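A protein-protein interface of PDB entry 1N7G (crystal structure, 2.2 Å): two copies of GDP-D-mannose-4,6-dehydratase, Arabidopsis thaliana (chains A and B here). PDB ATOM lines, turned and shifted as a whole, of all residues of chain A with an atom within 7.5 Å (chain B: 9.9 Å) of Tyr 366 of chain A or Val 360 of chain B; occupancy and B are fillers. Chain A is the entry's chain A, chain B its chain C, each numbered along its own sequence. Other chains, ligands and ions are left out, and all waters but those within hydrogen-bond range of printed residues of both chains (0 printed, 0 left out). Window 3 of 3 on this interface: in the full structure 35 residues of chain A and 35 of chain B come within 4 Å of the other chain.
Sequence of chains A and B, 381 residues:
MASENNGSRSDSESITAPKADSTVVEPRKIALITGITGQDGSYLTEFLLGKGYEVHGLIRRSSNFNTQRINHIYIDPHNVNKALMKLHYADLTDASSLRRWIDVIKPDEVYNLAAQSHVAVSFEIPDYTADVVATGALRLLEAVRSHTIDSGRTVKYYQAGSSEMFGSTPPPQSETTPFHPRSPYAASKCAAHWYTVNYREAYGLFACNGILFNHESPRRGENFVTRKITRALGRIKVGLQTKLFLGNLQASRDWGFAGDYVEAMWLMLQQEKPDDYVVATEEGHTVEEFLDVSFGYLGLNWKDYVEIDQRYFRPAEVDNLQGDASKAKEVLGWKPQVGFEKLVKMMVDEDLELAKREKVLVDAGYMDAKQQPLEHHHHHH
Val 360 of chain A touches Tyr 366 of chain B (CG1 to OH, 3.7 Å). CD2 of Leu 361 of chain B touches CD2 of Leu 361 of chain A, at 3.4 Å. Gly 365 of chain A touches Arg 357 of chain B. Tyr 366 of chain A touches Arg 357 of chain B (CE2 to CB, 3.4 Å). Val 360 of chain B touches Tyr 366 of chain A (CB to OH, 3.3 Å). Leu 361 of chain B touches Tyr 366 of chain A.
Val 360 of chain A touches Tyr 366 of chain B, and with the chains exchanged Tyr 366 of chain A touches Val 360 of chain B. Leu 361 of chain A touches its own counterpart, Leu 361 of chain B. Tyr 366 of chain A touches Leu 361 of chain B, but with the chains exchanged Leu 361 of chain A does not touch Tyr 366 of chain B (4.2 Å). Of the 6 pairs that touch across the chains among the printed residues, 3 have their exchanged pair printed and touching as well.
Of the 9 printed residues of chain A, 4 touch a printed residue of chain B. Of the 18 printed residues of chain B, 4 touch a printed residue of chain A. Hydrophobic or aromatic side chains of chain B within 4 Å of the printed part of chain A: Val 360, Leu 361 and Tyr 366. Among the printed residues, 6 pairs touch across the chains. Among the printed residues, no Asp or Glu carboxylate lies within 4 Å of a Lys or Arg side-chain nitrogen of the other chain.
Of chain B, only Arg 357, Val 360 and Leu 361 come within 4 Å of Tyr 366 of chain A. Of chain B, only Arg 357 (3.6 Å) comes within 4 Å of Gly 365 of chain A. No residue of chain B comes within 4 Å of Met 367 of chain A. Of the printed residues of chain B, Val 360 of chain A touches Tyr 366 (3.7 Å). Printed residues of chain A within 4 Å of Leu 361 of chain B: Leu 361 (3.4 Å) and Tyr 366 (3.9 Å). Leu 354 of chain B touches none of the printed residues of chain A. Asp 363 of chain A touches none of the printed residues of chain B.
N of Tyr 366 of chain A lies within hydrogen-bond range of O of Leu 361 of chain A (2.9 Å). O of Leu 361 of chain A lies within hydrogen-bond range of N of Met 367 of chain A (3.4 Å). OE2 of Glu 353 of chain B is in salt-bridge range of NE of Arg 357 of chain B, at 3.4 Å. The backbone carbonyl oxygen (O) of Leu 361 of chain B is in hydrogen-bond range of the backbone NH (N) of Tyr 366 of chain B. The backbone carbonyl oxygen of Leu 361 of chain B is in hydrogen-bond range of the backbone NH of Met 367 of chain B.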
ATOM      1  N   GLU A 358      26.829 -17.756 -13.995  1.00  0.00           N
ATOM      2  CA  GLU A 358      25.553 -17.120 -13.672  1.00  0.00           C
ATOM      3  C   GLU A 358      25.813 -15.774 -13.005  1.00  0.00           C
ATOM      4  O   GLU A 358      25.211 -14.765 -13.359  1.00  0.00           O
ATOM      5  CB  GLU A 358      24.723 -18.004 -12.733  1.00  0.00           C
ATOM      6  CG  GLU A 358      24.070 -19.199 -13.406  1.00  0.00           C
ATOM      7  CD  GLU A 358      23.186 -19.995 -12.460  1.00  0.00           C
ATOM      8  OE1 GLU A 358      22.450 -20.879 -12.946  1.00  0.00           O
ATOM      9  OE2 GLU A 358      23.224 -19.743 -11.235  1.00  0.00           O
ATOM     10  N   VAL A 360      28.218 -13.849 -13.308  1.00  0.00           N
ATOM     11  CA  VAL A 360      28.631 -12.898 -14.327  1.00  0.00           C
ATOM     12  C   VAL A 360      27.421 -12.360 -15.085  1.00  0.00           C
ATOM     13  O   VAL A 360      27.322 -11.161 -15.340  1.00  0.00           O
ATOM     14  CB  VAL A 360      29.602 -13.549 -15.327  1.00  0.00           C
ATOM     15  CG1 VAL A 360      29.987 -12.549 -16.407  1.00  0.00           C
ATOM     16  CG2 VAL A 360      30.837 -14.044 -14.593  1.00  0.00           C
ATOM     17  N   LEU A 361      26.496 -13.246 -15.437  1.00  0.00           N
ATOM     18  CA  LEU A 361      25.307 -12.832 -16.169  1.00  0.00           C
ATOM     19  C   LEU A 361      24.352 -12.026 -15.290  1.00  0.00           C
ATOM     20  O   LEU A 361      23.522 -11.267 -15.791  1.00  0.00           O
ATOM     21  CB  LEU A 361      24.594 -14.054 -16.747  1.00  0.00           C
ATOM     22  CG  LEU A 361      25.444 -14.910 -17.694  1.00  0.00           C
ATOM     23  CD1 LEU A 361      24.570 -15.973 -18.329  1.00  0.00           C
ATOM     24  CD2 LEU A 361      26.076 -14.042 -18.773  1.00  0.00           C
ATOM     25  N   VAL A 362      24.477 -12.189 -13.977  1.00  0.00           N
ATOM     26  CA  VAL A 362      23.628 -11.459 -13.050  1.00  0.00           C
ATOM     27  C   VAL A 362      24.131 -10.033 -12.937  1.00  0.00           C
ATOM     28  O   VAL A 362      23.368  -9.080 -13.070  1.00  0.00           O
ATOM     29  CB  VAL A 362      23.643 -12.101 -11.649  1.00  0.00           C
ATOM     30  CG1 VAL A 362      23.019 -11.153 -10.632  1.00  0.00           C
ATOM     31  CG2 VAL A 362      22.882 -13.418 -11.681  1.00  0.00           C
ATOM     32  N   ASP A 363      25.428  -9.901 -12.694  1.00  0.00           N
ATOM     33  CA  ASP A 363      26.057  -8.595 -12.559  1.00  0.00           C
ATOM     34  C   ASP A 363      26.144  -7.877 -13.904  1.00  0.00           C
ATOM     35  O   ASP A 363      26.805  -6.847 -14.021  1.00  0.00           O
ATOM     36  CB  ASP A 363      27.461  -8.754 -11.968  1.00  0.00           C
ATOM     37  CG  ASP A 363      27.454  -9.468 -10.627  1.00  0.00           C
ATOM     38  OD1 ASP A 363      28.550  -9.751 -10.096  1.00  0.00           O
ATOM     39  OD2 ASP A 363      26.352  -9.746 -10.103  1.00  0.00           O
ATOM     40  N   ALA A 364      25.481  -8.425 -14.920  1.00  0.00           N
ATOM     41  CA  ALA A 364      25.495  -7.819 -16.247  1.00  0.00           C
ATOM     42  C   ALA A 364      24.087  -7.458 -16.693  1.00  0.00           C
ATOM     43  O   ALA A 364      23.902  -6.755 -17.683  1.00  0.00           O
ATOM     44  CB  ALA A 364      26.133  -8.766 -17.252  1.00  0.00           C
ATOM     45  N   GLY A 365      23.093  -7.949 -15.962  1.00  0.00           N
ATOM     46  CA  GLY A 365      21.713  -7.656 -16.303  1.00  0.00           C
ATOM     47  C   GLY A 365      21.068  -8.662 -17.236  1.00  0.00           C
ATOM     48  O   GLY A 365      19.909  -8.498 -17.625  1.00  0.00           O
ATOM     49  N   TYR A 366      21.807  -9.706 -17.600  1.00  0.00           N
ATOM     50  CA  TYR A 366      21.282 -10.730 -18.495  1.00  0.00           C
ATOM     51  C   TYR A 366      20.225 -11.613 -17.838  1.00  0.00           C
ATOM     52  O   TYR A 366      19.371 -12.178 -18.523  1.00  0.00           O
ATOM     53  CB  TYR A 366      22.426 -11.591 -19.037  1.00  0.00           C
ATOM     54  CG  TYR A 366      23.114 -10.977 -20.234  1.00  0.00           C
ATOM     55  CD1 TYR A 366      23.530  -9.644 -20.218  1.00  0.00           C
ATOM     56  CD2 TYR A 366      23.340 -11.723 -21.391  1.00  0.00           C
ATOM     57  CE1 TYR A 366      24.148  -9.068 -21.326  1.00  0.00           C
ATOM     58  CE2 TYR A 366      23.959 -11.158 -22.505  1.00  0.00           C
ATOM     59  CZ  TYR A 366      24.359  -9.829 -22.466  1.00  0.00           C
ATOM     60  OH  TYR A 366      24.956  -9.260 -23.568  1.00  0.00           O
ATOM     61  N   MET A 367      20.282 -11.726 -16.512  1.00  0.00           N
ATOM     62  CA  MET A 367      19.322 -12.536 -15.767  1.00  0.00           C
ATOM     63  C   MET A 367      19.126 -12.019 -14.342  1.00  0.00           C
ATOM     64  O   MET A 367      19.793 -11.028 -13.975  1.00  0.00           O
ATOM     65  CB  MET A 367      19.774 -14.004 -15.726  1.00  0.00           C
ATOM     66  CG  MET A 367      21.202 -14.218 -15.231  1.00  0.00           C
ATOM     67  SD  MET A 367      21.592 -15.960 -14.900  1.00  0.00           S
ATOM     68  CE  MET A 367      21.737 -16.630 -16.561  1.00  0.00           C
ATOM     69  N   VAL B 238      21.381 -10.565 -36.417  1.00  0.00           N
ATOM     70  CA  VAL B 238      22.677 -10.520 -35.747  1.00  0.00           C
ATOM     71  C   VAL B 238      23.679 -11.498 -36.348  1.00  0.00           C
ATOM     72  O   VAL B 238      24.809 -11.603 -35.876  1.00  0.00           O
ATOM     73  CB  VAL B 238      22.549 -10.809 -34.231  1.00  0.00           C
ATOM     74  CG1 VAL B 238      21.686  -9.743 -33.572  1.00  0.00           C
ATOM     75  CG2 VAL B 238      21.964 -12.199 -34.006  1.00  0.00           C
ATOM     76  N   LEU B 240      23.245 -14.816 -36.511  1.00  0.00           N
ATOM     77  CA  LEU B 240      23.147 -16.129 -35.882  1.00  0.00           C
ATOM     78  C   LEU B 240      22.419 -17.147 -36.749  1.00  0.00           C
ATOM     79  O   LEU B 240      22.664 -18.348 -36.642  1.00  0.00           O
ATOM     80  CB  LEU B 240      22.434 -16.020 -34.529  1.00  0.00           C
ATOM     81  CG  LEU B 240      23.226 -15.401 -33.376  1.00  0.00           C
ATOM     82  CD1 LEU B 240      22.349 -15.299 -32.136  1.00  0.00           C
ATOM     83  CD2 LEU B 240      24.457 -16.256 -33.092  1.00  0.00           C
ATOM     84  N   LEU B 352      14.900  -9.490 -30.750  1.00  0.00           N
ATOM     85  CA  LEU B 352      16.113  -8.902 -31.318  1.00  0.00           C
ATOM     86  C   LEU B 352      17.100  -8.743 -30.176  1.00  0.00           C
ATOM     87  O   LEU B 352      18.262  -9.141 -30.278  1.00  0.00           O
ATOM     88  CB  LEU B 352      15.839  -7.529 -31.936  1.00  0.00           C
ATOM     89  CG  LEU B 352      17.098  -6.872 -32.522  1.00  0.00           C
ATOM     90  CD1 LEU B 352      17.616  -7.722 -33.681  1.00  0.00           C
ATOM     91  CD2 LEU B 352      16.789  -5.452 -32.995  1.00  0.00           C
ATOM     92  N   GLU B 353      16.622  -8.159 -29.081  1.00  0.00           N
ATOM     93  CA  GLU B 353      17.445  -7.963 -27.902  1.00  0.00           C
ATOM     94  C   GLU B 353      17.875  -9.322 -27.364  1.00  0.00           C
ATOM     95  O   GLU B 353      18.967  -9.467 -26.813  1.00  0.00           O
ATOM     96  CB  GLU B 353      16.660  -7.213 -26.827  1.00  0.00           C
ATOM     97  CG  GLU B 353      17.449  -6.953 -25.558  1.00  0.00           C
ATOM     98  CD  GLU B 353      18.739  -6.183 -25.819  1.00  0.00           C
ATOM     99  OE1 GLU B 353      18.680  -5.129 -26.493  1.00  0.00           O
ATOM    100  OE2 GLU B 353      19.809  -6.630 -25.347  1.00  0.00           O
ATOM    101  N   LEU B 354      17.009 -10.318 -27.530  1.00  0.00           N
ATOM    102  CA  LEU B 354      17.307 -11.662 -27.057  1.00  0.00           C
ATOM    103  C   LEU B 354      18.408 -12.248 -27.924  1.00  0.00           C
ATOM    104  O   LEU B 354      19.347 -12.862 -27.421  1.00  0.00           O
ATOM    105  CB  LEU B 354      16.064 -12.555 -27.140  1.00  0.00           C
ATOM    106  CG  LEU B 354      15.893 -13.606 -26.035  1.00  0.00           C
ATOM    107  CD1 LEU B 354      14.768 -14.557 -26.427  1.00  0.00           C
ATOM    108  CD2 LEU B 354      17.189 -14.386 -25.818  1.00  0.00           C
ATOM    109  N   ALA B 355      18.290 -12.056 -29.232  1.00  0.00           N
ATOM    110  CA  ALA B 355      19.284 -12.575 -30.161  1.00  0.00           C
ATOM    111  C   ALA B 355      20.641 -11.912 -29.941  1.00  0.00           C
ATOM    112  O   ALA B 355      21.677 -12.566 -30.045  1.00  0.00           O
ATOM    113  CB  ALA B 355      18.820 -12.360 -31.594  1.00  0.00           C
ATOM    114  N   LYS B 356      20.631 -10.616 -29.632  1.00  0.00           N
ATOM    115  CA  LYS B 356      21.864  -9.867 -29.400  1.00  0.00           C
ATOM    116  C   LYS B 356      22.593 -10.392 -28.168  1.00  0.00           C
ATOM    117  O   LYS B 356      23.809 -10.591 -28.199  1.00  0.00           O
ATOM    118  CB  LYS B 356      21.559  -8.376 -29.233  1.00  0.00           C
ATOM    119  N   ARG B 357      21.852 -10.609 -27.084  1.00  0.00           N
ATOM    120  CA  ARG B 357      22.446 -11.125 -25.853  1.00  0.00           C
ATOM    121  C   ARG B 357      23.041 -12.501 -26.120  1.00  0.00           C
ATOM    122  O   ARG B 357      24.097 -12.847 -25.594  1.00  0.00           O
ATOM    123  CB  ARG B 357      21.402 -11.227 -24.742  1.00  0.00           C
ATOM    124  CG  ARG B 357      20.823  -9.897 -24.322  1.00  0.00           C
ATOM    125  CD  ARG B 357      19.956 -10.051 -23.085  1.00  0.00           C
ATOM    126  NE  ARG B 357      19.297  -8.799 -22.719  1.00  0.00           N
ATOM    127  CZ  ARG B 357      18.582  -8.630 -21.611  1.00  0.00           C
ATOM    128  NH1 ARG B 357      18.434  -9.632 -20.752  1.00  0.00           N
ATOM    129  NH2 ARG B 357      18.006  -7.462 -21.367  1.00  0.00           N
ATOM    130  N   GLU B 358      22.355 -13.286 -26.941  1.00  0.00           N
ATOM    131  CA  GLU B 358      22.846 -14.609 -27.279  1.00  0.00           C
ATOM    132  C   GLU B 358      24.171 -14.461 -28.000  1.00  0.00           C
ATOM    133  O   GLU B 358      25.161 -15.093 -27.628  1.00  0.00           O
ATOM    134  CB  GLU B 358      21.856 -15.347 -28.179  1.00  0.00           C
ATOM    135  CG  GLU B 358      20.636 -15.864 -27.447  1.00  0.00           C
ATOM    136  CD  GLU B 358      19.704 -16.652 -28.347  1.00  0.00           C
ATOM    137  OE1 GLU B 358      18.736 -17.225 -27.815  1.00  0.00           O
ATOM    138  OE2 GLU B 358      19.936 -16.700 -29.578  1.00  0.00           O
ATOM    139  N   LYS B 359      24.185 -13.618 -29.028  1.00  0.00           N
ATOM    140  CA  LYS B 359      25.394 -13.386 -29.803  1.00  0.00           C
ATOM    141  C   LYS B 359      26.549 -13.042 -28.870  1.00  0.00           C
ATOM    142  O   LYS B 359      27.660 -13.557 -29.026  1.00  0.00           O
ATOM    143  CB  LYS B 359      25.183 -12.250 -30.808  1.00  0.00           C
ATOM    144  CG  LYS B 359      26.343 -12.094 -31.781  1.00  0.00           C
ATOM    145  CD  LYS B 359      26.145 -10.926 -32.729  1.00  0.00           C
ATOM    146  CE  LYS B 359      27.343 -10.769 -33.663  1.00  0.00           C
ATOM    147  NZ  LYS B 359      27.160  -9.645 -34.631  1.00  0.00           N
ATOM    148  N   VAL B 360      26.284 -12.173 -27.898  1.00  0.00           N
ATOM    149  CA  VAL B 360      27.305 -11.783 -26.938  1.00  0.00           C
ATOM    150  C   VAL B 360      27.804 -13.000 -26.155  1.00  0.00           C
ATOM    151  O   VAL B 360      29.009 -13.184 -25.993  1.00  0.00           O
ATOM    152  CB  VAL B 360      26.774 -10.721 -25.939  1.00  0.00           C
ATOM    153  CG1 VAL B 360      27.786 -10.507 -24.808  1.00  0.00           C
ATOM    154  CG2 VAL B 360      26.533  -9.401 -26.664  1.00  0.00           C
ATOM    155  N   LEU B 361      26.881 -13.833 -25.679  1.00  0.00           N
ATOM    156  CA  LEU B 361      27.263 -15.016 -24.915  1.00  0.00           C
ATOM    157  C   LEU B 361      27.995 -16.034 -25.778  1.00  0.00           C
ATOM    158  O   LEU B 361      28.898 -16.720 -25.302  1.00  0.00           O
ATOM    159  CB  LEU B 361      26.036 -15.664 -24.273  1.00  0.00           C
ATOM    160  CG  LEU B 361      25.295 -14.809 -23.244  1.00  0.00           C
ATOM    161  CD1 LEU B 361      24.153 -15.623 -22.639  1.00  0.00           C
ATOM    162  CD2 LEU B 361      26.261 -14.346 -22.160  1.00  0.00           C
ATOM    163  N   VAL B 362      27.606 -16.139 -27.044  1.00  0.00           N
ATOM    164  CA  VAL B 362      28.265 -17.068 -27.951  1.00  0.00           C
ATOM    165  C   VAL B 362      29.666 -16.543 -28.264  1.00  0.00           C
ATOM    166  O   VAL B 362      30.644 -17.294 -28.241  1.00  0.00           O
ATOM    167  CB  VAL B 362      27.496 -17.205 -29.274  1.00  0.00           C
ATOM    168  CG1 VAL B 362      28.187 -18.227 -30.172  1.00  0.00           C
ATOM    169  CG2 VAL B 362      26.055 -17.610 -28.998  1.00  0.00           C
ATOM    170  N   ASP B 363      29.752 -15.245 -28.555  1.00  0.00           N
ATOM    171  CA  ASP B 363      31.025 -14.611 -28.877  1.00  0.00           C
ATOM    172  C   ASP B 363      31.997 -14.689 -27.707  1.00  0.00           C
ATOM    173  O   ASP B 363      33.199 -14.846 -27.902  1.00  0.00           O
ATOM    174  CB  ASP B 363      30.802 -13.146 -29.270  1.00  0.00           C
ATOM    175  CG  ASP B 363      30.289 -12.989 -30.693  1.00  0.00           C
ATOM    176  OD1 ASP B 363      29.813 -11.886 -31.041  1.00  0.00           O
ATOM    177  OD2 ASP B 363      30.372 -13.965 -31.468  1.00  0.00           O
ATOM    178  N   ALA B 364      31.471 -14.587 -26.492  1.00  0.00           N
ATOM    179  CA  ALA B 364      32.295 -14.639 -25.291  1.00  0.00           C
ATOM    180  C   ALA B 364      32.581 -16.066 -24.818  1.00  0.00           C
ATOM    181  O   ALA B 364      33.231 -16.266 -23.792  1.00  0.00           O
ATOM    182  CB  ALA B 364      31.626 -13.847 -24.179  1.00  0.00           C
ATOM    183  N   GLY B 365      32.091 -17.054 -25.560  1.00  0.00           N
ATOM    184  CA  GLY B 365      32.323 -18.440 -25.187  1.00  0.00           C
ATOM    185  C   GLY B 365      31.474 -18.924 -24.025  1.00  0.00           C
ATOM    186  O   GLY B 365      31.900 -19.785 -23.257  1.00  0.00           O
ATOM    187  N   TYR B 366      30.272 -18.375 -23.894  1.00  0.00           N
ATOM    188  CA  TYR B 366      29.365 -18.770 -22.823  1.00  0.00           C
ATOM    189  C   TYR B 366      28.265 -19.700 -23.318  1.00  0.00           C
ATOM    190  O   TYR B 366      27.619 -20.375 -22.521  1.00  0.00           O
ATOM    191  CB  TYR B 366      28.741 -17.541 -22.169  1.00  0.00           C
ATOM    192  CG  TYR B 366      29.609 -16.912 -21.109  1.00  0.00           C
ATOM    193  CD1 TYR B 366      30.911 -16.511 -21.393  1.00  0.00           C
ATOM    194  CD2 TYR B 366      29.122 -16.708 -19.819  1.00  0.00           C
ATOM    195  CE1 TYR B 366      31.713 -15.919 -20.418  1.00  0.00           C
ATOM    196  CE2 TYR B 366      29.911 -16.119 -18.835  1.00  0.00           C
ATOM    197  CZ  TYR B 366      31.205 -15.725 -19.141  1.00  0.00           C
ATOM    198  OH  TYR B 366      31.987 -15.131 -18.174  1.00  0.00           O
ATOM    199  N   MET B 367      28.047 -19.724 -24.629  1.00  0.00           N
ATOM    200  CA  MET B 367      27.034 -20.593 -25.217  1.00  0.00           C
ATOM    201  C   MET B 367      27.645 -21.329 -26.398  1.00  0.00           C
ATOM    202  O   MET B 367      28.715 -20.882 -26.860  1.00  0.00           O
ATOM    203  CB  MET B 367      25.822 -19.785 -25.699  1.00  0.00           C
ATOM    204  CG  MET B 367      25.009 -19.118 -24.599  1.00  0.00           C
ATOM    205  SD  MET B 367      23.453 -18.416 -25.220  1.00  0.00           S
ATOM    206  CE  MET B 367      22.273 -19.636 -24.633  1.00  0.00           C
